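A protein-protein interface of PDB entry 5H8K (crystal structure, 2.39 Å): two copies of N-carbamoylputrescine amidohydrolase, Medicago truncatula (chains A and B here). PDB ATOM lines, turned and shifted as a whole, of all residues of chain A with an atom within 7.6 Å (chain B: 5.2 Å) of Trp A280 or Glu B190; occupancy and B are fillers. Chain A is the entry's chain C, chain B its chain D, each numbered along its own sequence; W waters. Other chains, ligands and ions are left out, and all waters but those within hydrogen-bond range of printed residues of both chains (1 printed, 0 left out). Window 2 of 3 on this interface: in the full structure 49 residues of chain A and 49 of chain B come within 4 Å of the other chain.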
ATOM      1  N   GLY A 211     -19.987 -37.384 -19.917  1.00  0.00           N
ATOM      2  CA  GLY A 211     -21.095 -36.793 -20.710  1.00  0.00           C
ATOM      3  C   GLY A 211     -21.610 -35.475 -20.192  1.00  0.00           C
ATOM      4  O   GLY A 211     -22.066 -34.635 -20.937  1.00  0.00           O
ATOM      5  N   ALA A 212     -21.474 -35.268 -18.894  1.00  0.00           N
ATOM      6  CA  ALA A 212     -22.048 -34.051 -18.246  1.00  0.00           C
ATOM      7  C   ALA A 212     -21.130 -32.841 -18.377  1.00  0.00           C
ATOM      8  O   ALA A 212     -21.581 -31.663 -18.305  1.00  0.00           O
ATOM      9  CB  ALA A 212     -22.321 -34.329 -16.768  1.00  0.00           C
ATOM     10  N   LEU A 214     -18.779 -32.950 -21.050  1.00  0.00           N
ATOM     11  CA  LEU A 214     -18.341 -32.999 -22.419  1.00  0.00           C
ATOM     12  C   LEU A 214     -16.824 -32.958 -22.507  1.00  0.00           C
ATOM     13  O   LEU A 214     -16.267 -32.131 -23.190  1.00  0.00           O
ATOM     14  CB  LEU A 214     -18.978 -31.870 -23.211  1.00  0.00           C
ATOM     15  CG  LEU A 214     -20.490 -32.081 -23.309  1.00  0.00           C
ATOM     16  CD1 LEU A 214     -21.251 -31.058 -22.513  1.00  0.00           C
ATOM     17  CD2 LEU A 214     -21.006 -32.059 -24.744  1.00  0.00           C
ATOM     18  N   PRO A 248     -16.475 -37.598 -25.197  1.00  0.00           N
ATOM     19  CA  PRO A 248     -17.193 -36.533 -24.464  1.00  0.00           C
ATOM     20  C   PRO A 248     -18.706 -36.581 -24.522  1.00  0.00           C
ATOM     21  O   PRO A 248     -19.369 -35.571 -24.182  1.00  0.00           O
ATOM     22  CB  PRO A 248     -16.723 -35.252 -25.157  1.00  0.00           C
ATOM     23  CG  PRO A 248     -16.519 -35.726 -26.613  1.00  0.00           C
ATOM     24  CD  PRO A 248     -15.859 -37.096 -26.436  1.00  0.00           C
ATOM     25  N   LYS A 274     -13.919 -28.792 -27.766  1.00  0.00           N
ATOM     26  CA  LYS A 274     -14.127 -27.555 -27.029  1.00  0.00           C
ATOM     27  C   LYS A 274     -15.345 -26.927 -27.644  1.00  0.00           C
ATOM     28  O   LYS A 274     -16.253 -26.438 -26.941  1.00  0.00           O
ATOM     29  CB  LYS A 274     -12.912 -26.610 -27.165  1.00  0.00           C
ATOM     30  CG  LYS A 274     -13.054 -25.255 -26.494  1.00  0.00           C
ATOM     31  CD  LYS A 274     -11.775 -24.426 -26.649  1.00  0.00           C
ATOM     32  CE  LYS A 274     -12.040 -22.929 -26.390  1.00  0.00           C
ATOM     33  NZ  LYS A 274     -10.941 -22.035 -26.827  1.00  0.00           N
ATOM     34  N   SER A 275     -15.361 -26.930 -28.954  1.00  0.00           N
ATOM     35  CA  SER A 275     -16.450 -26.268 -29.646  1.00  0.00           C
ATOM     36  C   SER A 275     -17.801 -26.939 -29.332  1.00  0.00           C
ATOM     37  O   SER A 275     -18.778 -26.274 -29.020  1.00  0.00           O
ATOM     38  CB  SER A 275     -16.166 -26.200 -31.126  1.00  0.00           C
ATOM     39  OG  SER A 275     -17.205 -25.519 -31.734  1.00  0.00           O
ATOM     40  N   MET A 276     -17.790 -28.262 -29.276  1.00  0.00           N
ATOM     41  CA  MET A 276     -18.961 -29.079 -28.952  1.00  0.00           C
ATOM     42  C   MET A 276     -19.418 -28.842 -27.524  1.00  0.00           C
ATOM     43  O   MET A 276     -20.593 -28.676 -27.256  1.00  0.00           O
ATOM     44  CB  MET A 276     -18.636 -30.583 -29.182  1.00  0.00           C
ATOM     45  CG  MET A 276     -19.670 -31.569 -28.648  1.00  0.00           C
ATOM     46  SD  MET A 276     -19.037 -33.255 -28.330  1.00  0.00           S
ATOM     47  CE  MET A 276     -18.422 -33.740 -29.971  1.00  0.00           C
ATOM     48  N   ARG A 277     -18.466 -28.842 -26.610  1.00  0.00           N
ATOM     49  CA  ARG A 277     -18.757 -28.650 -25.199  1.00  0.00           C
ATOM     50  C   ARG A 277     -19.496 -27.311 -24.996  1.00  0.00           C
ATOM     51  O   ARG A 277     -20.470 -27.258 -24.261  1.00  0.00           O
ATOM     52  CB  ARG A 277     -17.472 -28.713 -24.391  1.00  0.00           C
ATOM     53  CG  ARG A 277     -17.569 -28.165 -22.938  1.00  0.00           C
ATOM     54  CD  ARG A 277     -16.361 -28.588 -22.141  1.00  0.00           C
ATOM     55  NE  ARG A 277     -15.079 -28.034 -22.609  1.00  0.00           N
ATOM     56  CZ  ARG A 277     -14.119 -28.747 -23.228  1.00  0.00           C
ATOM     57  NH1 ARG A 277     -14.344 -30.027 -23.570  1.00  0.00           N
ATOM     58  NH2 ARG A 277     -12.976 -28.171 -23.568  1.00  0.00           N
ATOM     59  N   HIS A 278     -19.053 -26.243 -25.671  1.00  0.00           N
ATOM     60  CA  HIS A 278     -19.651 -24.916 -25.490  1.00  0.00           C
ATOM     61  C   HIS A 278     -20.996 -24.791 -26.171  1.00  0.00           C
ATOM     62  O   HIS A 278     -21.912 -24.200 -25.651  1.00  0.00           O
ATOM     63  CB  HIS A 278     -18.721 -23.830 -26.032  1.00  0.00           C
ATOM     64  CG  HIS A 278     -17.458 -23.689 -25.244  1.00  0.00           C
ATOM     65  ND1 HIS A 278     -16.406 -22.898 -25.644  1.00  0.00           N
ATOM     66  CD2 HIS A 278     -17.075 -24.255 -24.076  1.00  0.00           C
ATOM     67  CE1 HIS A 278     -15.423 -22.983 -24.766  1.00  0.00           C
ATOM     68  NE2 HIS A 278     -15.806 -23.803 -23.803  1.00  0.00           N
ATOM     69  N   CYS A 279     -21.175 -25.340 -27.351  1.00  0.00           N
ATOM     70  CA  CYS A 279     -22.450 -25.276 -28.013  1.00  0.00           C
ATOM     71  C   CYS A 279     -23.536 -26.109 -27.307  1.00  0.00           C
ATOM     72  O   CYS A 279     -24.734 -25.830 -27.428  1.00  0.00           O
ATOM     73  CB  CYS A 279     -22.266 -25.766 -29.438  1.00  0.00           C
ATOM     74  SG  CYS A 279     -23.749 -25.620 -30.417  1.00  0.00           S
ATOM     75  N   TRP A 280     -23.144 -27.176 -26.597  1.00  0.00           N
ATOM     76  CA  TRP A 280     -24.194 -27.953 -25.935  1.00  0.00           C
ATOM     77  C   TRP A 280     -24.820 -27.114 -24.820  1.00  0.00           C
ATOM     78  O   TRP A 280     -26.018 -27.194 -24.538  1.00  0.00           O
ATOM     79  CB  TRP A 280     -23.707 -29.257 -25.357  1.00  0.00           C
ATOM     80  CG  TRP A 280     -24.807 -30.228 -25.022  1.00  0.00           C
ATOM     81  CD1 TRP A 280     -25.024 -30.799 -23.809  1.00  0.00           C
ATOM     82  CD2 TRP A 280     -25.812 -30.777 -25.910  1.00  0.00           C
ATOM     83  NE1 TRP A 280     -26.089 -31.639 -23.865  1.00  0.00           N
ATOM     84  CE2 TRP A 280     -26.584 -31.666 -25.148  1.00  0.00           C
ATOM     85  CE3 TRP A 280     -26.116 -30.609 -27.269  1.00  0.00           C
ATOM     86  CZ2 TRP A 280     -27.670 -32.348 -25.671  1.00  0.00           C
ATOM     87  CZ3 TRP A 280     -27.209 -31.276 -27.803  1.00  0.00           C
ATOM     88  CH2 TRP A 280     -27.987 -32.132 -27.005  1.00  0.00           C
ATOM     89  N   GLY A 281     -23.991 -26.286 -24.196  1.00  0.00           N
ATOM     90  CA  GLY A 281     -24.474 -25.180 -23.396  1.00  0.00           C
ATOM     91  C   GLY A 281     -24.589 -25.412 -21.907  1.00  0.00           C
ATOM     92  O   GLY A 281     -25.012 -24.506 -21.171  1.00  0.00           O
ATOM     93  N   VAL A 282     -24.205 -26.581 -21.418  1.00  0.00           N
ATOM     94  CA  VAL A 282     -24.491 -26.822 -20.034  1.00  0.00           C
ATOM     95  C   VAL A 282     -23.748 -25.812 -19.119  1.00  0.00           C
ATOM     96  O   VAL A 282     -24.318 -25.387 -18.088  1.00  0.00           O
ATOM     97  CB  VAL A 282     -24.223 -28.262 -19.604  1.00  0.00           C
ATOM     98  CG1 VAL A 282     -25.292 -29.180 -20.170  1.00  0.00           C
ATOM     99  CG2 VAL A 282     -22.836 -28.733 -19.999  1.00  0.00           C
ATOM    100  N   PHE A 283     -22.522 -25.407 -19.510  1.00  0.00           N
ATOM    101  CA  PHE A 283     -21.704 -24.484 -18.706  1.00  0.00           C
ATOM    102  C   PHE A 283     -22.255 -23.042 -18.748  1.00  0.00           C
ATOM    103  O   PHE A 283     -21.970 -22.253 -17.844  1.00  0.00           O
ATOM    104  CB  PHE A 283     -20.246 -24.516 -19.136  1.00  0.00           C
ATOM    105  CG  PHE A 283     -19.539 -25.764 -18.713  1.00  0.00           C
ATOM    106  CD1 PHE A 283     -19.121 -25.924 -17.411  1.00  0.00           C
ATOM    107  CD2 PHE A 283     -19.354 -26.834 -19.615  1.00  0.00           C
ATOM    108  CE1 PHE A 283     -18.481 -27.076 -16.995  1.00  0.00           C
ATOM    109  CE2 PHE A 283     -18.718 -27.997 -19.207  1.00  0.00           C
ATOM    110  CZ  PHE A 283     -18.280 -28.131 -17.889  1.00  0.00           C
ATOM    111  N   ARG A 284     -23.023 -22.720 -19.781  1.00  0.00           N
ATOM    112  CA  ARG A 284     -23.681 -21.402 -19.950  1.00  0.00           C
ATOM    113  C   ARG A 284     -24.925 -21.355 -19.053  1.00  0.00           C
ATOM    114  O   ARG A 284     -25.390 -20.317 -18.671  1.00  0.00           O
ATOM    115  CB  ARG A 284     -24.114 -21.233 -21.425  1.00  0.00           C
ATOM    116  CG  ARG A 284     -24.893 -19.981 -21.782  1.00  0.00           C
ATOM    117  CD  ARG A 284     -25.688 -20.107 -23.081  1.00  0.00           C
ATOM    118  NE  ARG A 284     -26.587 -21.249 -22.929  1.00  0.00           N
ATOM    119  CZ  ARG A 284     -27.003 -22.012 -23.931  1.00  0.00           C
ATOM    120  NH1 ARG A 284     -26.697 -21.702 -25.166  1.00  0.00           N
ATOM    121  NH2 ARG A 284     -27.750 -23.084 -23.684  1.00  0.00           N
ATOM    122  N   ASP A 285     -25.474 -22.527 -18.746  1.00  0.00           N
ATOM    123  CA  ASP A 285     -26.749 -22.599 -18.086  1.00  0.00           C
ATOM    124  C   ASP A 285     -26.664 -23.021 -16.635  1.00  0.00           C
ATOM    125  O   ASP A 285     -27.684 -23.063 -15.977  1.00  0.00           O
ATOM    126  CB  ASP A 285     -27.603 -23.605 -18.830  1.00  0.00           C
ATOM    127  CG  ASP A 285     -27.868 -23.210 -20.291  1.00  0.00           C
ATOM    128  OD1 ASP A 285     -27.692 -22.009 -20.663  1.00  0.00           O
ATOM    129  OD2 ASP A 285     -28.273 -24.101 -21.070  1.00  0.00           O
ATOM    130  N   PRO B 131     -31.721 -23.453 -31.531  1.00  0.00           N
ATOM    131  CA  PRO B 131     -32.723 -23.803 -32.535  1.00  0.00           C
ATOM    132  C   PRO B 131     -33.551 -25.002 -32.088  1.00  0.00           C
ATOM    133  O   PRO B 131     -33.013 -26.022 -31.648  1.00  0.00           O
ATOM    134  CB  PRO B 131     -31.884 -24.140 -33.736  1.00  0.00           C
ATOM    135  CG  PRO B 131     -30.720 -23.212 -33.592  1.00  0.00           C
ATOM    136  CD  PRO B 131     -30.389 -23.371 -32.123  1.00  0.00           C
ATOM    137  N   TYR B 133     -35.359 -25.180 -29.348  1.00  0.00           N
ATOM    138  CA  TYR B 133     -35.457 -25.254 -27.899  1.00  0.00           C
ATOM    139  C   TYR B 133     -35.177 -23.870 -27.280  1.00  0.00           C
ATOM    140  O   TYR B 133     -34.318 -23.695 -26.401  1.00  0.00           O
ATOM    141  CB  TYR B 133     -34.511 -26.332 -27.322  1.00  0.00           C
ATOM    142  CG  TYR B 133     -34.718 -27.679 -27.898  1.00  0.00           C
ATOM    143  CD1 TYR B 133     -34.140 -28.024 -29.111  1.00  0.00           C
ATOM    144  CD2 TYR B 133     -35.526 -28.612 -27.266  1.00  0.00           C
ATOM    145  CE1 TYR B 133     -34.335 -29.266 -29.675  1.00  0.00           C
ATOM    146  CE2 TYR B 133     -35.740 -29.876 -27.844  1.00  0.00           C
ATOM    147  CZ  TYR B 133     -35.141 -30.201 -29.052  1.00  0.00           C
ATOM    148  OH  TYR B 133     -35.359 -31.425 -29.669  1.00  0.00           O
ATOM    149  N   TRP B 162     -34.232 -30.376 -19.090  1.00  0.00           N
ATOM    150  CA  TRP B 162     -32.830 -29.921 -19.134  1.00  0.00           C
ATOM    151  C   TRP B 162     -32.125 -29.970 -17.786  1.00  0.00           C
ATOM    152  O   TRP B 162     -30.936 -30.227 -17.768  1.00  0.00           O
ATOM    153  CB  TRP B 162     -32.753 -28.520 -19.753  1.00  0.00           C
ATOM    154  CG  TRP B 162     -31.417 -27.975 -20.146  1.00  0.00           C
ATOM    155  CD1 TRP B 162     -30.855 -26.807 -19.682  1.00  0.00           C
ATOM    156  CD2 TRP B 162     -30.506 -28.465 -21.157  1.00  0.00           C
ATOM    157  NE1 TRP B 162     -29.644 -26.573 -20.299  1.00  0.00           N
ATOM    158  CE2 TRP B 162     -29.414 -27.551 -21.219  1.00  0.00           C
ATOM    159  CE3 TRP B 162     -30.500 -29.575 -22.012  1.00  0.00           C
ATOM    160  CZ2 TRP B 162     -28.330 -27.736 -22.063  1.00  0.00           C
ATOM    161  CZ3 TRP B 162     -29.405 -29.758 -22.876  1.00  0.00           C
ATOM    162  CH2 TRP B 162     -28.343 -28.848 -22.894  1.00  0.00           C
ATOM    163  N   TRP B 165     -29.506 -32.802 -17.205  1.00  0.00           N
ATOM    164  CA  TRP B 165     -28.110 -32.857 -17.616  1.00  0.00           C
ATOM    165  C   TRP B 165     -27.114 -32.452 -16.496  1.00  0.00           C
ATOM    166  O   TRP B 165     -25.921 -32.605 -16.661  1.00  0.00           O
ATOM    167  CB  TRP B 165     -27.891 -31.967 -18.857  1.00  0.00           C
ATOM    168  CG  TRP B 165     -28.623 -32.518 -20.107  1.00  0.00           C
ATOM    169  CD1 TRP B 165     -29.906 -32.293 -20.431  1.00  0.00           C
ATOM    170  CD2 TRP B 165     -28.116 -33.420 -21.101  1.00  0.00           C
ATOM    171  NE1 TRP B 165     -30.253 -32.967 -21.594  1.00  0.00           N
ATOM    172  CE2 TRP B 165     -29.167 -33.671 -22.023  1.00  0.00           C
ATOM    173  CE3 TRP B 165     -26.866 -34.020 -21.326  1.00  0.00           C
ATOM    174  CZ2 TRP B 165     -29.017 -34.449 -23.127  1.00  0.00           C
ATOM    175  CZ3 TRP B 165     -26.721 -34.836 -22.447  1.00  0.00           C
ATOM    176  CH2 TRP B 165     -27.803 -35.024 -23.331  1.00  0.00           C
ATOM    177  N   ILE B 187     -37.364 -33.968 -25.379  1.00  0.00           N
ATOM    178  CA  ILE B 187     -36.144 -33.849 -26.184  1.00  0.00           C
ATOM    179  C   ILE B 187     -36.262 -34.762 -27.415  1.00  0.00           C
ATOM    180  O   ILE B 187     -36.828 -35.852 -27.326  1.00  0.00           O
ATOM    181  CB  ILE B 187     -34.943 -34.195 -25.306  1.00  0.00           C
ATOM    182  CG1 ILE B 187     -33.647 -33.798 -25.968  1.00  0.00           C
ATOM    183  CG2 ILE B 187     -34.927 -35.674 -24.917  1.00  0.00           C
ATOM    184  CD1 ILE B 187     -32.433 -33.849 -25.030  1.00  0.00           C
ATOM    185  N   GLY B 188     -35.804 -34.270 -28.569  1.00  0.00           N
ATOM    186  CA  GLY B 188     -35.808 -34.998 -29.813  1.00  0.00           C
ATOM    187  C   GLY B 188     -34.685 -34.568 -30.719  1.00  0.00           C
ATOM    188  O   GLY B 188     -33.601 -34.209 -30.263  1.00  0.00           O
ATOM    189  N   SER B 189     -34.941 -34.624 -32.014  1.00  0.00           N
ATOM    190  CA  SER B 189     -34.060 -34.037 -33.033  1.00  0.00           C
ATOM    191  C   SER B 189     -33.918 -32.491 -32.882  1.00  0.00           C
ATOM    192  O   SER B 189     -34.650 -31.840 -32.129  1.00  0.00           O
ATOM    193  CB  SER B 189     -34.589 -34.381 -34.444  1.00  0.00           C
ATOM    194  OG  SER B 189     -35.919 -33.925 -34.555  1.00  0.00           O
ATOM    195  N   GLU B 190     -32.957 -31.939 -33.607  1.00  0.00           N
ATOM    196  CA  GLU B 190     -32.694 -30.521 -33.581  1.00  0.00           C
ATOM    197  C   GLU B 190     -32.743 -29.996 -34.988  1.00  0.00           C
ATOM    198  O   GLU B 190     -32.075 -30.541 -35.869  1.00  0.00           O
ATOM    199  CB  GLU B 190     -31.338 -30.239 -32.959  1.00  0.00           C
ATOM    200  CG  GLU B 190     -31.145 -31.047 -31.721  1.00  0.00           C
ATOM    201  CD  GLU B 190     -30.310 -30.298 -30.708  1.00  0.00           C
ATOM    202  OE1 GLU B 190     -29.935 -29.144 -30.997  1.00  0.00           O
ATOM    203  OE2 GLU B 190     -30.041 -30.859 -29.622  1.00  0.00           O
ATOM    204  N   PRO B 191     -33.563 -28.956 -35.208  1.00  0.00           N
ATOM    205  CA  PRO B 191     -33.966 -28.575 -36.551  1.00  0.00           C
ATOM    206  C   PRO B 191     -32.856 -27.904 -37.344  1.00  0.00           C
ATOM    207  O   PRO B 191     -32.961 -27.825 -38.558  1.00  0.00           O
ATOM    208  CB  PRO B 191     -35.115 -27.603 -36.302  1.00  0.00           C
ATOM    209  CG  PRO B 191     -34.916 -27.090 -34.926  1.00  0.00           C
ATOM    210  CD  PRO B 191     -34.345 -28.251 -34.178  1.00  0.00           C
ATOM    211  N   HIS B 192     -31.804 -27.404 -36.669  1.00  0.00           N
ATOM    212  CA  HIS B 192     -30.699 -26.809 -37.454  1.00  0.00           C
ATOM    213  C   HIS B 192     -29.646 -27.810 -37.933  1.00  0.00           C
ATOM    214  O   HIS B 192     -28.795 -27.429 -38.729  1.00  0.00           O
ATOM    215  CB  HIS B 192     -29.983 -25.690 -36.682  1.00  0.00           C
ATOM    216  CG  HIS B 192     -29.235 -26.187 -35.488  1.00  0.00           C
ATOM    217  ND1 HIS B 192     -29.840 -26.923 -34.493  1.00  0.00           N
ATOM    218  CD2 HIS B 192     -27.931 -26.086 -35.141  1.00  0.00           C
ATOM    219  CE1 HIS B 192     -28.942 -27.244 -33.577  1.00  0.00           C
ATOM    220  NE2 HIS B 192     -27.774 -26.765 -33.955  1.00  0.00           N
ATOM    221  N   ASP B 193     -29.678 -29.045 -37.411  1.00  0.00           N
ATOM    222  CA  ASP B 193     -28.663 -30.100 -37.711  1.00  0.00           C
ATOM    223  C   ASP B 193     -29.244 -31.504 -37.544  1.00  0.00           C
ATOM    224  O   ASP B 193     -29.376 -32.046 -36.428  1.00  0.00           O
ATOM    225  CB  ASP B 193     -27.455 -29.931 -36.791  1.00  0.00           C
ATOM    226  CG  ASP B 193     -26.299 -30.773 -37.196  1.00  0.00           C
ATOM    227  OD1 ASP B 193     -26.498 -31.656 -38.016  1.00  0.00           O
ATOM    228  OD2 ASP B 193     -25.190 -30.575 -36.653  1.00  0.00           O
ATOM    229  N   GLN B 194     -29.611 -32.091 -38.670  1.00  0.00           N
ATOM    230  CA  GLN B 194     -30.183 -33.450 -38.640  1.00  0.00           C
ATOM    231  C   GLN B 194     -29.183 -34.577 -38.165  1.00  0.00           C
ATOM    232  O   GLN B 194     -29.614 -35.652 -37.785  1.00  0.00           O
ATOM    233  CB  GLN B 194     -30.812 -33.772 -39.984  1.00  0.00           C
ATOM    234  CG  GLN B 194     -29.813 -33.672 -41.117  1.00  0.00           C
ATOM    235  CD  GLN B 194     -30.476 -33.796 -42.512  1.00  0.00           C
ATOM    236  OE1 GLN B 194     -31.289 -32.946 -42.931  1.00  0.00           O
ATOM    237  NE2 GLN B 194     -30.136 -34.875 -43.223  1.00  0.00           N
ATOM    238  N   ILE B 196     -27.458 -34.430 -35.393  1.00  0.00           N
ATOM    239  CA  ILE B 196     -27.404 -34.513 -33.940  1.00  0.00           C
ATOM    240  C   ILE B 196     -28.463 -35.505 -33.435  1.00  0.00           C
ATOM    241  O   ILE B 196     -29.689 -35.308 -33.692  1.00  0.00           O
ATOM    242  CB  ILE B 196     -27.727 -33.167 -33.257  1.00  0.00           C
ATOM    243  CG1 ILE B 196     -26.664 -32.093 -33.535  1.00  0.00           C
ATOM    244  CG2 ILE B 196     -27.947 -33.388 -31.775  1.00  0.00           C
ATOM    245  CD1 ILE B 196     -27.128 -30.679 -33.121  1.00  0.00           C
ATOM    246  N   SER B 198     -29.099 -37.067 -29.724  1.00  0.00           N
ATOM    247  CA  SER B 198     -28.640 -36.946 -28.372  1.00  0.00           C
ATOM    248  C   SER B 198     -29.040 -38.115 -27.459  1.00  0.00           C
ATOM    249  O   SER B 198     -28.596 -38.165 -26.321  1.00  0.00           O
ATOM    250  CB  SER B 198     -29.122 -35.623 -27.820  1.00  0.00           C
ATOM    251  OG  SER B 198     -30.509 -35.525 -27.752  1.00  0.00           O
ATOM    252  N   HIS B 201     -26.377 -40.119 -25.225  1.00  0.00           N
ATOM    253  CA  HIS B 201     -25.697 -39.147 -24.391  1.00  0.00           C
ATOM    254  C   HIS B 201     -26.605 -38.770 -23.219  1.00  0.00           C
ATOM    255  O   HIS B 201     -26.182 -38.794 -22.053  1.00  0.00           O
ATOM    256  CB  HIS B 201     -25.363 -37.972 -25.282  1.00  0.00           C
ATOM    257  CG  HIS B 201     -24.612 -36.907 -24.617  1.00  0.00           C
ATOM    258  ND1 HIS B 201     -24.618 -35.613 -25.075  1.00  0.00           N
ATOM    259  CD2 HIS B 201     -23.804 -36.920 -23.534  1.00  0.00           C
ATOM    260  CE1 HIS B 201     -23.836 -34.876 -24.316  1.00  0.00           C
ATOM    261  NE2 HIS B 201     -23.337 -35.642 -23.367  1.00  0.00           N
HETATM  262  O   HOH W   1     -23.779 -30.808 -17.147  1.00  0.00           O
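OD1 of Asp A285 is in salt-bridge range of NE of Arg A284, 2.6 Å away.
Among the printed residues, no Asp or Glu carboxylate lies within 4 Å of a Lys or Arg side-chain nitrogen of the other chain.
Water W1 lies within hydrogen-bond range of O of Ala A212 and O of Trp B165.
Among the printed residues, merely in contact across the chains: Trp A280 with Trp B162 (3.3 Å), Trp A280 with Glu B190 (3.4 Å), Trp A280 with Trp B165 (3.6 Å), Trp A280 with Ser B198 (3.8 Å), Val A282 with Trp B162 (3.9 Å), Trp A280 with His B201 (3.97 Å) and Ala A212 with Trp B165 (3.99 Å).
The side-chain carboxylate of Asp A285 sits at hydrogen-bond distance from the indole nitrogen of Trp B162 (2.9 Å).
The backbone carbonyl oxygen (O) of Gly A211 lies within hydrogen-bond range of a ring nitrogen (NE2) of His B201, 2.9 Å away.
Of chain B, only Trp B162 (3.3 Å), Trp B165 (3.6 Å), Glu B190 (3.4 Å), Ser B198 (3.8 Å) and His B201 (3.97 Å) come within 4 Å of Trp A280.
Printed residues of chain B within 4 Å of Val A282: Trp B162.
Phe A283 touches none of the printed residues of chain B.
Printed residues of chain B within 4 Å of Asp A285: Trp B162.
Ile B187 touches none of the printed residues of chain A.
Glu B190 touches just one residue of chain A: Trp A280 (3.4 Å).
The nearest residue of chain B that does not touch Trp A280 is Ile B196 (4.6 Å).
The nearest printed residue of chain A that does not touch Glu B190 is Cys A279 (7.1 Å).
No position is printed for both chains.
Of the 9 pairs that touch across the chains among the printed residues, none has its exchanged pair printed and touching as well.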
